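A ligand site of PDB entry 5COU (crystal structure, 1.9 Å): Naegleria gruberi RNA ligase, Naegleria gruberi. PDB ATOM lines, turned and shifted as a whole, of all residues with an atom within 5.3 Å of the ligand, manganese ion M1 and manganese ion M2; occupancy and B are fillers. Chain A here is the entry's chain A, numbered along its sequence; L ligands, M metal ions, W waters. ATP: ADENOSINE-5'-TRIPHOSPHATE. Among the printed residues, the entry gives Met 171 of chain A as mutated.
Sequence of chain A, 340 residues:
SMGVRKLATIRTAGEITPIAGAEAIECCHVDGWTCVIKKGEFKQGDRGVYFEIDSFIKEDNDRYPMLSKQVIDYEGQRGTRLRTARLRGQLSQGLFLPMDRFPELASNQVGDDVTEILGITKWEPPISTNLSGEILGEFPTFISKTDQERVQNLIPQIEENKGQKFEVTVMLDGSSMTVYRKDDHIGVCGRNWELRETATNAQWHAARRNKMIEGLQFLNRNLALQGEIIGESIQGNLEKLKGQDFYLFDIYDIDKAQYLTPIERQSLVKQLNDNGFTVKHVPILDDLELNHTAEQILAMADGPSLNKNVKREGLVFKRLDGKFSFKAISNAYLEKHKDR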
ATOM      1  N   ARG A   5     -24.406  14.545  -2.707  1.00  0.00           N
ATOM      2  CA  ARG A   5     -25.355  15.682  -2.849  1.00  0.00           C
ATOM      3  C   ARG A   5     -26.703  15.340  -2.197  1.00  0.00           C
ATOM      4  O   ARG A   5     -27.204  14.208  -2.323  1.00  0.00           O
ATOM      5  CB  ARG A   5     -25.561  15.972  -4.356  1.00  0.00           C
ATOM      6  CG  ARG A   5     -26.488  17.121  -4.713  1.00  0.00           C
ATOM      7  CD  ARG A   5     -26.235  17.565  -6.131  1.00  0.00           C
ATOM      8  NE  ARG A   5     -27.401  18.233  -6.638  1.00  0.00           N
ATOM      9  CZ  ARG A   5     -27.781  18.190  -7.914  1.00  0.00           C
ATOM     10  NH1 ARG A   5     -27.013  17.594  -8.823  1.00  0.00           N
ATOM     11  NH2 ARG A   5     -28.940  18.758  -8.269  1.00  0.00           N
ATOM     12  N   ASP A  54     -31.475  16.069 -11.618  1.00  0.00           N
ATOM     13  CA  ASP A  54     -30.349  15.093 -11.516  1.00  0.00           C
ATOM     14  C   ASP A  54     -30.673  13.883 -10.653  1.00  0.00           C
ATOM     15  O   ASP A  54     -29.966  12.859 -10.715  1.00  0.00           O
ATOM     16  CB  ASP A  54     -28.972  15.665 -11.163  1.00  0.00           C
ATOM     17  CG  ASP A  54     -28.600  16.895 -11.956  1.00  0.00           C
ATOM     18  OD1 ASP A  54     -29.176  17.178 -13.038  1.00  0.00           O
ATOM     19  OD2 ASP A  54     -27.718  17.663 -11.450  1.00  0.00           O
ATOM     20  N   LYS A 122     -27.615   9.707  -8.171  1.00  0.00           N
ATOM     21  CA  LYS A 122     -27.422  10.938  -8.919  1.00  0.00           C
ATOM     22  C   LYS A 122     -27.203  10.604 -10.404  1.00  0.00           C
ATOM     23  O   LYS A 122     -26.224   9.929 -10.729  1.00  0.00           O
ATOM     24  CB  LYS A 122     -26.206  11.699  -8.423  1.00  0.00           C
ATOM     25  CG  LYS A 122     -26.240  13.177  -8.906  1.00  0.00           C
ATOM     26  CD  LYS A 122     -25.130  14.033  -8.301  1.00  0.00           C
ATOM     27  CE  LYS A 122     -23.956  13.898  -9.239  1.00  0.00           C
ATOM     28  NZ  LYS A 122     -23.167  15.132  -9.208  1.00  0.00           N
ATOM     29  N   PRO A 125     -24.141  13.634 -16.664  1.00  0.00           N
ATOM     30  CA  PRO A 125     -23.673  13.523 -18.068  1.00  0.00           C
ATOM     31  C   PRO A 125     -22.489  12.592 -18.101  1.00  0.00           C
ATOM     32  O   PRO A 125     -21.852  12.404 -17.110  1.00  0.00           O
ATOM     33  CB  PRO A 125     -23.156  14.913 -18.372  1.00  0.00           C
ATOM     34  CG  PRO A 125     -23.919  15.838 -17.456  1.00  0.00           C
ATOM     35  CD  PRO A 125     -24.132  15.031 -16.185  1.00  0.00           C
ATOM     36  N   THR A 146     -13.831  20.860  -5.863  1.00  0.00           N
ATOM     37  CA  THR A 146     -14.510  22.060  -6.358  1.00  0.00           C
ATOM     38  C   THR A 146     -16.015  21.778  -6.259  1.00  0.00           C
ATOM     39  O   THR A 146     -16.518  20.727  -6.685  1.00  0.00           O
ATOM     40  CB  THR A 146     -14.101  22.476  -7.796  1.00  0.00           C
ATOM     41  OG1 THR A 146     -14.417  21.404  -8.730  1.00  0.00           O
ATOM     42  CG2 THR A 146     -12.573  22.718  -7.831  1.00  0.00           C
ATOM     43  N   ASP A 147     -16.722  22.682  -5.653  1.00  0.00           N
ATOM     44  CA  ASP A 147     -18.153  22.418  -5.406  1.00  0.00           C
ATOM     45  C   ASP A 147     -18.733  23.781  -5.162  1.00  0.00           C
ATOM     46  O   ASP A 147     -18.077  24.612  -4.514  1.00  0.00           O
ATOM     47  CB  ASP A 147     -18.326  21.457  -4.194  1.00  0.00           C
ATOM     48  CG  ASP A 147     -19.739  21.436  -3.648  1.00  0.00           C
ATOM     49  OD1 ASP A 147     -20.120  22.411  -2.944  1.00  0.00           O
ATOM     50  OD2 ASP A 147     -20.473  20.448  -3.940  1.00  0.00           O
ATOM     51  N   GLN A 148     -19.959  24.019  -5.680  1.00  0.00           N
ATOM     52  CA  GLN A 148     -20.758  25.228  -5.415  1.00  0.00           C
ATOM     53  C   GLN A 148     -22.192  24.822  -5.204  1.00  0.00           C
ATOM     54  O   GLN A 148     -22.761  24.064  -5.979  1.00  0.00           O
ATOM     55  CB  GLN A 148     -20.723  26.229  -6.567  1.00  0.00           C
ATOM     56  CG  GLN A 148     -19.291  26.572  -6.991  1.00  0.00           C
ATOM     57  CD  GLN A 148     -18.670  27.484  -5.974  1.00  0.00           C
ATOM     58  OE1 GLN A 148     -19.379  27.964  -5.067  1.00  0.00           O
ATOM     59  NE2 GLN A 148     -17.346  27.737  -6.094  1.00  0.00           N
ATOM     60  N   ARG A 150     -26.216  25.548  -5.247  1.00  0.00           N
ATOM     61  CA  ARG A 150     -27.171  26.270  -6.066  1.00  0.00           C
ATOM     62  C   ARG A 150     -27.899  27.337  -5.264  1.00  0.00           C
ATOM     63  O   ARG A 150     -28.312  27.087  -4.119  1.00  0.00           O
ATOM     64  CB  ARG A 150     -28.191  25.216  -6.611  1.00  0.00           C
ATOM     65  CG  ARG A 150     -27.599  24.349  -7.742  1.00  0.00           C
ATOM     66  CD  ARG A 150     -28.570  23.243  -8.232  1.00  0.00           C
ATOM     67  NE  ARG A 150     -27.996  22.532  -9.409  1.00  0.00           N
ATOM     68  CZ  ARG A 150     -27.079  21.552  -9.353  1.00  0.00           C
ATOM     69  NH1 ARG A 150     -26.577  21.111  -8.170  1.00  0.00           N
ATOM     70  NH2 ARG A 150     -26.658  20.999 -10.500  1.00  0.00           N
ATOM     71  N   THR A 169     -18.100  35.564 -11.736  1.00  0.00           N
ATOM     72  CA  THR A 169     -17.408  35.002 -12.873  1.00  0.00           C
ATOM     73  C   THR A 169     -18.354  34.170 -13.747  1.00  0.00           C
ATOM     74  O   THR A 169     -19.343  33.604 -13.240  1.00  0.00           O
ATOM     75  CB  THR A 169     -16.233  34.120 -12.462  1.00  0.00           C
ATOM     76  OG1 THR A 169     -16.698  33.125 -11.568  1.00  0.00           O
ATOM     77  CG2 THR A 169     -15.115  34.987 -11.735  1.00  0.00           C
ATOM     78  N   VAL A 170     -17.988  34.040 -15.027  1.00  0.00           N
ATOM     79  CA  VAL A 170     -18.751  33.154 -15.921  1.00  0.00           C
ATOM     80  C   VAL A 170     -18.454  31.688 -15.544  1.00  0.00           C
ATOM     81  O   VAL A 170     -17.299  31.350 -15.332  1.00  0.00           O
ATOM     82  CB  VAL A 170     -18.402  33.428 -17.404  1.00  0.00           C
ATOM     83  CG1 VAL A 170     -19.103  32.417 -18.304  1.00  0.00           C
ATOM     84  CG2 VAL A 170     -18.774  34.867 -17.819  1.00  0.00           C
ATOM     85  N   MET A 171     -19.525  30.891 -15.385  1.00  0.00           N
ATOM     86  CA  MET A 171     -19.440  29.484 -15.166  1.00  0.00           C
ATOM     87  C   MET A 171     -19.185  28.819 -16.538  1.00  0.00           C
ATOM     88  O   MET A 171     -20.055  28.844 -17.437  1.00  0.00           O
ATOM     89  CB  MET A 171     -20.766  28.964 -14.640  1.00  0.00           C
ATOM     90  CG  MET A 171     -20.746  27.494 -14.272  1.00  0.00           C
ATOM     91  SD  MET A 171     -22.300  27.041 -13.386  1.00  0.00           S
ATOM     92  CE  MET A 171     -21.854  25.322 -13.079  1.00  0.00           C
ATOM     93  N   LEU A 172     -17.992  28.289 -16.719  1.00  0.00           N
ATOM     94  CA  LEU A 172     -17.656  27.518 -17.931  1.00  0.00           C
ATOM     95  C   LEU A 172     -18.084  26.056 -17.807  1.00  0.00           C
ATOM     96  O   LEU A 172     -17.896  25.425 -16.778  1.00  0.00           O
ATOM     97  CB  LEU A 172     -16.131  27.558 -18.190  1.00  0.00           C
ATOM     98  CG  LEU A 172     -15.557  28.924 -18.365  1.00  0.00           C
ATOM     99  CD1 LEU A 172     -14.093  28.826 -18.768  1.00  0.00           C
ATOM    100  CD2 LEU A 172     -16.409  29.687 -19.392  1.00  0.00           C
ATOM    101  N   ASP A 173     -18.615  25.491 -18.890  1.00  0.00           N
ATOM    102  CA  ASP A 173     -19.013  24.083 -18.917  1.00  0.00           C
ATOM    103  C   ASP A 173     -17.915  23.198 -19.446  1.00  0.00           C
ATOM    104  O   ASP A 173     -17.798  22.948 -20.701  1.00  0.00           O
ATOM    105  CB  ASP A 173     -20.251  23.927 -19.827  1.00  0.00           C
ATOM    106  CG  ASP A 173     -20.984  22.628 -19.622  1.00  0.00           C
ATOM    107  OD1 ASP A 173     -20.456  21.672 -19.007  1.00  0.00           O
ATOM    108  OD2 ASP A 173     -22.149  22.538 -20.107  1.00  0.00           O
ATOM    109  N   GLY A 174     -17.090  22.685 -18.542  1.00  0.00           N
ATOM    110  CA  GLY A 174     -16.025  21.789 -19.010  1.00  0.00           C
ATOM    111  C   GLY A 174     -15.834  20.722 -17.962  1.00  0.00           C
ATOM    112  O   GLY A 174     -16.791  20.095 -17.592  1.00  0.00           O
ATOM    113  N   SER A 175     -14.605  20.530 -17.502  1.00  0.00           N
ATOM    114  CA  SER A 175     -14.333  19.557 -16.472  1.00  0.00           C
ATOM    115  C   SER A 175     -13.443  20.270 -15.440  1.00  0.00           C
ATOM    116  O   SER A 175     -12.464  20.937 -15.844  1.00  0.00           O
ATOM    117  CB  SER A 175     -13.552  18.370 -17.009  1.00  0.00           C
ATOM    118  OG  SER A 175     -13.675  17.298 -16.107  1.00  0.00           O
ATOM    119  N   SER A 176     -13.727  20.093 -14.139  1.00  0.00           N
ATOM    120  CA  SER A 176     -12.863  20.635 -13.081  1.00  0.00           C
ATOM    121  C   SER A 176     -11.485  19.994 -13.105  1.00  0.00           C
ATOM    122  O   SER A 176     -11.343  18.769 -13.236  1.00  0.00           O
ATOM    123  CB  SER A 176     -13.457  20.336 -11.673  1.00  0.00           C
ATOM    124  OG  SER A 176     -12.644  20.847 -10.659  1.00  0.00           O
ATOM    125  N   GLY A 227      -9.469  25.011 -11.674  1.00  0.00           N
ATOM    126  CA  GLY A 227     -10.078  25.661 -12.815  1.00  0.00           C
ATOM    127  C   GLY A 227     -10.829  24.692 -13.657  1.00  0.00           C
ATOM    128  O   GLY A 227     -10.925  23.486 -13.280  1.00  0.00           O
ATOM    129  N   GLU A 228     -11.294  25.175 -14.810  1.00  0.00           N
ATOM    130  CA  GLU A 228     -12.080  24.369 -15.697  1.00  0.00           C
ATOM    131  C   GLU A 228     -11.180  24.136 -16.915  1.00  0.00           C
ATOM    132  O   GLU A 228     -10.686  25.097 -17.472  1.00  0.00           O
ATOM    133  CB  GLU A 228     -13.333  25.125 -16.149  1.00  0.00           C
ATOM    134  CG  GLU A 228     -14.444  24.200 -16.690  1.00  0.00           C
ATOM    135  CD  GLU A 228     -15.113  23.417 -15.542  1.00  0.00           C
ATOM    136  OE1 GLU A 228     -14.677  23.590 -14.335  1.00  0.00           O
ATOM    137  OE2 GLU A 228     -16.191  22.809 -15.822  1.00  0.00           O
ATOM    138  N   PHE A 249     -10.316  29.388 -11.595  1.00  0.00           N
ATOM    139  CA  PHE A 249     -11.419  30.065 -10.899  1.00  0.00           C
ATOM    140  C   PHE A 249     -11.165  30.183  -9.416  1.00  0.00           C
ATOM    141  O   PHE A 249     -11.862  30.968  -8.750  1.00  0.00           O
ATOM    142  CB  PHE A 249     -12.876  29.477 -11.208  1.00  0.00           C
ATOM    143  CG  PHE A 249     -12.964  27.961 -11.083  1.00  0.00           C
ATOM    144  CD1 PHE A 249     -12.866  27.338  -9.847  1.00  0.00           C
ATOM    145  CD2 PHE A 249     -13.160  27.165 -12.193  1.00  0.00           C
ATOM    146  CE1 PHE A 249     -12.945  25.937  -9.757  1.00  0.00           C
ATOM    147  CE2 PHE A 249     -13.142  25.776 -12.124  1.00  0.00           C
ATOM    148  CZ  PHE A 249     -13.066  25.160 -10.895  1.00  0.00           C
ATOM    149  N   ASP A 250     -10.245  29.381  -8.875  1.00  0.00           N
ATOM    150  CA  ASP A 250      -9.950  29.359  -7.460  1.00  0.00           C
ATOM    151  C   ASP A 250      -8.501  28.941  -7.179  1.00  0.00           C
ATOM    152  O   ASP A 250      -7.879  28.238  -7.937  1.00  0.00           O
ATOM    153  CB  ASP A 250     -10.804  28.325  -6.674  1.00  0.00           C
ATOM    154  CG  ASP A 250     -12.053  28.971  -6.027  1.00  0.00           C
ATOM    155  OD1 ASP A 250     -11.924  30.057  -5.431  1.00  0.00           O
ATOM    156  OD2 ASP A 250     -13.152  28.374  -6.151  1.00  0.00           O
ATOM    157  N   VAL A 282     -11.123  32.449 -15.571  1.00  0.00           N
ATOM    158  CA  VAL A 282     -12.518  32.425 -16.099  1.00  0.00           C
ATOM    159  C   VAL A 282     -12.915  33.889 -16.251  1.00  0.00           C
ATOM    160  O   VAL A 282     -12.446  34.740 -15.497  1.00  0.00           O
ATOM    161  CB  VAL A 282     -13.549  31.752 -15.140  1.00  0.00           C
ATOM    162  CG1 VAL A 282     -13.377  30.233 -15.057  1.00  0.00           C
ATOM    163  CG2 VAL A 282     -13.464  32.409 -13.771  1.00  0.00           C
ATOM    164  N   GLU A 313     -23.418  28.915 -19.317  1.00  0.00           N
ATOM    165  CA  GLU A 313     -24.010  27.932 -18.428  1.00  0.00           C
ATOM    166  C   GLU A 313     -24.557  28.690 -17.212  1.00  0.00           C
ATOM    167  O   GLU A 313     -25.627  28.336 -16.681  1.00  0.00           O
ATOM    168  CB  GLU A 313     -22.946  26.966 -17.874  1.00  0.00           C
ATOM    169  CG  GLU A 313     -23.590  25.809 -17.142  1.00  0.00           C
ATOM    170  CD  GLU A 313     -22.635  24.749 -16.650  1.00  0.00           C
ATOM    171  OE1 GLU A 313     -23.150  23.685 -16.186  1.00  0.00           O
ATOM    172  OE2 GLU A 313     -21.390  24.966 -16.642  1.00  0.00           O
ATOM    173  N   VAL A 316     -20.905  32.223 -11.260  1.00  0.00           N
ATOM    174  CA  VAL A 316     -20.475  31.795  -9.958  1.00  0.00           C
ATOM    175  C   VAL A 316     -20.150  33.083  -9.180  1.00  0.00           C
ATOM    176  O   VAL A 316     -19.519  33.978  -9.699  1.00  0.00           O
ATOM    177  CB  VAL A 316     -19.290  30.761 -10.011  1.00  0.00           C
ATOM    178  CG1 VAL A 316     -18.809  30.417  -8.605  1.00  0.00           C
ATOM    179  CG2 VAL A 316     -19.751  29.469 -10.701  1.00  0.00           C
ATOM    180  N   LYS A 318     -18.528  34.607  -5.581  1.00  0.00           N
ATOM    181  CA  LYS A 318     -17.603  34.245  -4.484  1.00  0.00           C
ATOM    182  C   LYS A 318     -17.459  35.529  -3.647  1.00  0.00           C
ATOM    183  O   LYS A 318     -17.147  36.621  -4.182  1.00  0.00           O
ATOM    184  CB  LYS A 318     -16.229  33.774  -5.040  1.00  0.00           C
ATOM    185  CG  LYS A 318     -16.321  32.481  -5.904  1.00  0.00           C
ATOM    186  CD  LYS A 318     -14.956  32.023  -6.502  1.00  0.00           C
ATOM    187  CE  LYS A 318     -15.109  30.981  -7.602  1.00  0.00           C
ATOM    188  NZ  LYS A 318     -15.639  31.679  -8.843  1.00  0.00           N
ATOM    189  N   LYS A 327     -23.359  28.954  -7.011  1.00  0.00           N
ATOM    190  CA  LYS A 327     -23.552  29.030  -8.467  1.00  0.00           C
ATOM    191  C   LYS A 327     -25.058  29.359  -8.784  1.00  0.00           C
ATOM    192  O   LYS A 327     -25.953  28.959  -8.040  1.00  0.00           O
ATOM    193  CB  LYS A 327     -23.115  27.723  -9.186  1.00  0.00           C
ATOM    194  CG  LYS A 327     -23.859  26.475  -8.660  1.00  0.00           C
ATOM    195  CD  LYS A 327     -23.352  25.144  -9.272  1.00  0.00           C
ATOM    196  CE  LYS A 327     -24.164  23.947  -8.750  1.00  0.00           C
ATOM    197  NZ  LYS A 327     -23.541  22.587  -8.886  1.00  0.00           N
ATOM    198  N   ILE A 329     -26.815  28.516 -12.094  1.00  0.00           N
ATOM    199  CA  ILE A 329     -26.984  27.912 -13.429  1.00  0.00           C
ATOM    200  C   ILE A 329     -28.161  28.546 -14.200  1.00  0.00           C
ATOM    201  O   ILE A 329     -29.293  28.591 -13.688  1.00  0.00           O
ATOM    202  CB  ILE A 329     -27.082  26.373 -13.338  1.00  0.00           C
ATOM    203  CG1 ILE A 329     -25.831  25.814 -12.596  1.00  0.00           C
ATOM    204  CG2 ILE A 329     -27.410  25.748 -14.697  1.00  0.00           C
ATOM    205  CD1 ILE A 329     -25.726  24.321 -12.396  1.00  0.00           C
HETATM  206  PG  ATP L   1     -23.774  18.923  -9.302  1.00  0.00           P
HETATM  207  O1G ATP L   1     -23.847  17.555  -8.719  1.00  0.00           O
HETATM  208  O2G ATP L   1     -24.105  19.963  -8.271  1.00  0.00           O
HETATM  209  O3G ATP L   1     -24.325  19.212 -10.641  1.00  0.00           O
HETATM  210  PB  ATP L   1     -21.209  19.379 -10.650  1.00  0.00           P
HETATM  211  O1B ATP L   1     -19.826  18.793 -10.264  1.00  0.00           O
HETATM  212  O2B ATP L   1     -21.823  19.125 -12.055  1.00  0.00           O
HETATM  213  O3B ATP L   1     -22.119  18.976  -9.391  1.00  0.00           O
HETATM  214  PA  ATP L   1     -21.305  22.198 -11.368  1.00  0.00           P
HETATM  215  O1A ATP L   1     -20.609  22.164 -12.700  1.00  0.00           O
HETATM  216  O2A ATP L   1     -22.794  22.387 -11.510  1.00  0.00           O
HETATM  217  O3A ATP L   1     -21.010  20.914 -10.489  1.00  0.00           O
HETATM  218  O5' ATP L   1     -20.820  23.351 -10.469  1.00  0.00           O
HETATM  219  C5' ATP L   1     -19.519  23.410  -9.839  1.00  0.00           C
HETATM  220  C4' ATP L   1     -18.383  23.314 -10.905  1.00  0.00           C
HETATM  221  O4' ATP L   1     -18.311  24.485 -11.726  1.00  0.00           O
HETATM  222  C3' ATP L   1     -16.980  23.272 -10.257  1.00  0.00           C
HETATM  223  O3' ATP L   1     -16.694  21.900  -9.904  1.00  0.00           O
HETATM  224  C2' ATP L   1     -16.077  23.724 -11.388  1.00  0.00           C
HETATM  225  O2' ATP L   1     -15.562  22.575 -12.123  1.00  0.00           O
HETATM  226  C1' ATP L   1     -16.971  24.502 -12.368  1.00  0.00           C
HETATM  227  N9  ATP L   1     -16.737  25.935 -12.694  1.00  0.00           N
HETATM  228  C8  ATP L   1     -16.884  26.470 -13.935  1.00  0.00           C
HETATM  229  N7  ATP L   1     -16.716  27.814 -13.874  1.00  0.00           N
HETATM  230  C5  ATP L   1     -16.542  28.136 -12.633  1.00  0.00           C
HETATM  231  C6  ATP L   1     -16.357  29.395 -11.933  1.00  0.00           C
HETATM  232  N6  ATP L   1     -16.388  30.532 -12.620  1.00  0.00           N
HETATM  233  N1  ATP L   1     -16.236  29.351 -10.582  1.00  0.00           N
HETATM  234  C2  ATP L   1     -16.235  28.187  -9.902  1.00  0.00           C
HETATM  235  N3  ATP L   1     -16.410  26.990 -10.498  1.00  0.00           N
HETATM  236  C4  ATP L   1     -16.598  26.915 -11.846  1.00  0.00           C
HETATM  237 MN    MN M   1     -23.825  18.761 -12.547  1.00  0.00          MN
HETATM  238 MN    MN M   2     -19.876  21.676 -14.635  1.00  0.00          MN
HETATM  239  O   HOH W   1     -25.817  18.548 -13.081  1.00  0.00           O
HETATM  240  O   HOH W   2     -19.738  23.424 -15.158  1.00  0.00           O
HETATM  241  O   HOH W   3     -23.586  17.112 -12.022  1.00  0.00           O
HETATM  242  O   HOH W   4     -16.052  25.575  -7.849  1.00  0.00           O
HETATM  243  O   HOH W   5     -23.142  18.101 -14.414  1.00  0.00           O
HETATM  244  O   HOH W   6     -18.898  20.195  -8.010  1.00  0.00           O
HETATM  245  O   HOH W   7     -21.869  21.681 -15.280  1.00  0.00           O
HETATM  246  O   HOH W   8     -19.350  21.086 -16.649  1.00  0.00           O
HETATM  247  O   HOH W   9     -18.974  16.570 -12.369  1.00  0.00           O
HETATM  248  O   HOH W  10     -17.194  19.374 -10.970  1.00  0.00           O
HETATM  249  O   HOH W  11     -23.089  20.491  -5.891  1.00  0.00           O
HETATM  250  O   HOH W  12     -24.053  20.331 -13.234  1.00  0.00           O
HETATM  251  O   HOH W  13     -22.534  17.003  -6.396  1.00  0.00           O
HETATM  252  O   HOH W  14     -19.905  19.832 -14.160  1.00  0.00           O
HETATM  253  O   HOH W  15     -17.774  21.511 -14.189  1.00  0.00           O
HETATM  254  O   HOH W  16     -21.051  21.819  -7.202  1.00  0.00           O
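No residue comes within 4 Å of manganese ion M2.
The nearest printed residue that does not touch manganese ion M2 is Glu 228 (4.03 Å).
The side-chain amino group of Lys 122 is in salt-bridge range of an oxygen (O1G) of the ligand (2.6 Å).
The side-chain carboxylate (OE1) of Glu 228 is in hydrogen-bond range of an oxygen (O2') of the ligand (2.6 Å).
The backbone carbonyl oxygen (O) of Thr 146 sits close to an oxygen (O3') of the ligand.
OG1 of Thr 146 is in hydrogen-bond range of O3' of the ligand (2.6 Å).
NH1 of Arg 150 lies within salt-bridge range of O2G of the ligand (2.7 Å).
O2A of the ligand lies within salt-bridge range of NZ of Lys 327, 2.7 Å away.
The side-chain hydroxyl (OG1) of Thr 169 is in hydrogen-bond range of a nitrogen (N6) of the ligand.
N1 of the ligand sits at hydrogen-bond distance from NZ of Lys 318, 3.0 Å away.
A nitrogen (N6) of the ligand is in hydrogen-bond range of the backbone carbonyl oxygen of Val 170, at 3.0 Å.
The backbone NH (N) of Leu 172 lies within hydrogen-bond range of a nitrogen (N7) of the ligand, 3.2 Å away.
NH1 of Arg 5 lies within salt-bridge range of O1G of the ligand (3.2 Å).
Manganese ion M2 is bound by water W2 (1.8 Å), water W14 (1.9 Å), water W7 (2.1 Å), O1A of the ligand (2.1 Å), water W15 (2.2 Å) and water W8 (2.2 Å).
Manganese ion M2 has six donor atoms within binding distance.
The side-chain carboxylate of Glu 228 is in hydrogen-bond range of the backbone NH of Gly 174, 2.9 Å away.
OE2 of Glu 228 lies within hydrogen-bond range of N of Ser 175 (3.2 Å).
The side-chain hydroxyl (OG) of Ser 176 is in hydrogen-bond range of the side-chain hydroxyl (OG1) of Thr 146, at 2.7 Å.
The guanidinium group (NH2) of Arg 150 is in salt-bridge range of the side-chain carboxylate (OD2) of Asp 54, 3.6 Å away.
NZ of Lys 327 lies close to O of Gln 148.
The side-chain hydroxyl (OG1) of Thr 169 sits at hydrogen-bond distance from the side-chain amino group (NZ) of Lys 318 (3.3 Å).
O of Thr 169 is in hydrogen-bond range of N of Val 316 (2.9 Å).
The guanidinium group (NH1) of Arg 5 is in salt-bridge range of the side-chain carboxylate (OD2) of Asp 54, at 2.7 Å.
No residue comes within 4 Å of manganese ion M1.
The nearest printed residue that does not touch manganese ion M1 is Arg 150 (4.2 Å).
Manganese ion M1 is bound by water W12, at 1.7 Å.
Water W3 is bound to manganese ion M1 (1.7 Å).
Manganese ion M1 is bound by an oxygen (O3G) of the ligand (2.0 Å).
Water W1 binds manganese ion M1 (2.1 Å).
An oxygen (O2B) of the ligand is bound to manganese ion M1 (2.1 Å).
Water W5 binds manganese ion M1, 2.1 Å away.
Residues that only touch the ligand: Asp 54 (3.8 Å), Gln 148 (3.99 Å), Met 171 (3.4 Å), Ser 176 (3.1 Å), Phe 249 (3.4 Å), Val 282 (3.7 Å), Val 316 (3.4 Å) and Ile 329 (3.6 Å).
Hydrophobic or aromatic side chains that line the ligand: Met 171, Phe 249, Val 282, Val 316 and Ile 329.
Within 4 Å of the ligand: Arg 5, Asp 54, Lys 122, Thr 146, Gln 148, Arg 150, Thr 169, Val 170, Met 171, Leu 172, Ser 176, Glu 228, Phe 249, Val 282, Val 316, Lys 318, Lys 327 and Ile 329.
Water W15 lies within hydrogen-bond range of the side-chain carboxylate (OE2) of Glu 228 and an oxygen (O2') of the ligand.
Water W2 lies within hydrogen-bond range of the side-chain carboxylate (OE2) of Glu 313 (2.7 Å) and the backbone carbonyl oxygen (O) of Leu 172 (3.2 Å).
Water W11 lies within hydrogen-bond range of an oxygen (O2G) of the ligand and the side-chain carboxylate of Asp 147.
Water W13 lies within hydrogen-bond range of an oxygen (O1G) of the ligand and the side-chain amino group of Lys 122.
Water W6 lies within hydrogen-bond range of O of Thr 146 and O1B of the ligand.
Water W4 lies within hydrogen-bond range of a nitrogen (N3) of the ligand and the side-chain amide nitrogen (NE2) of Gln 148.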
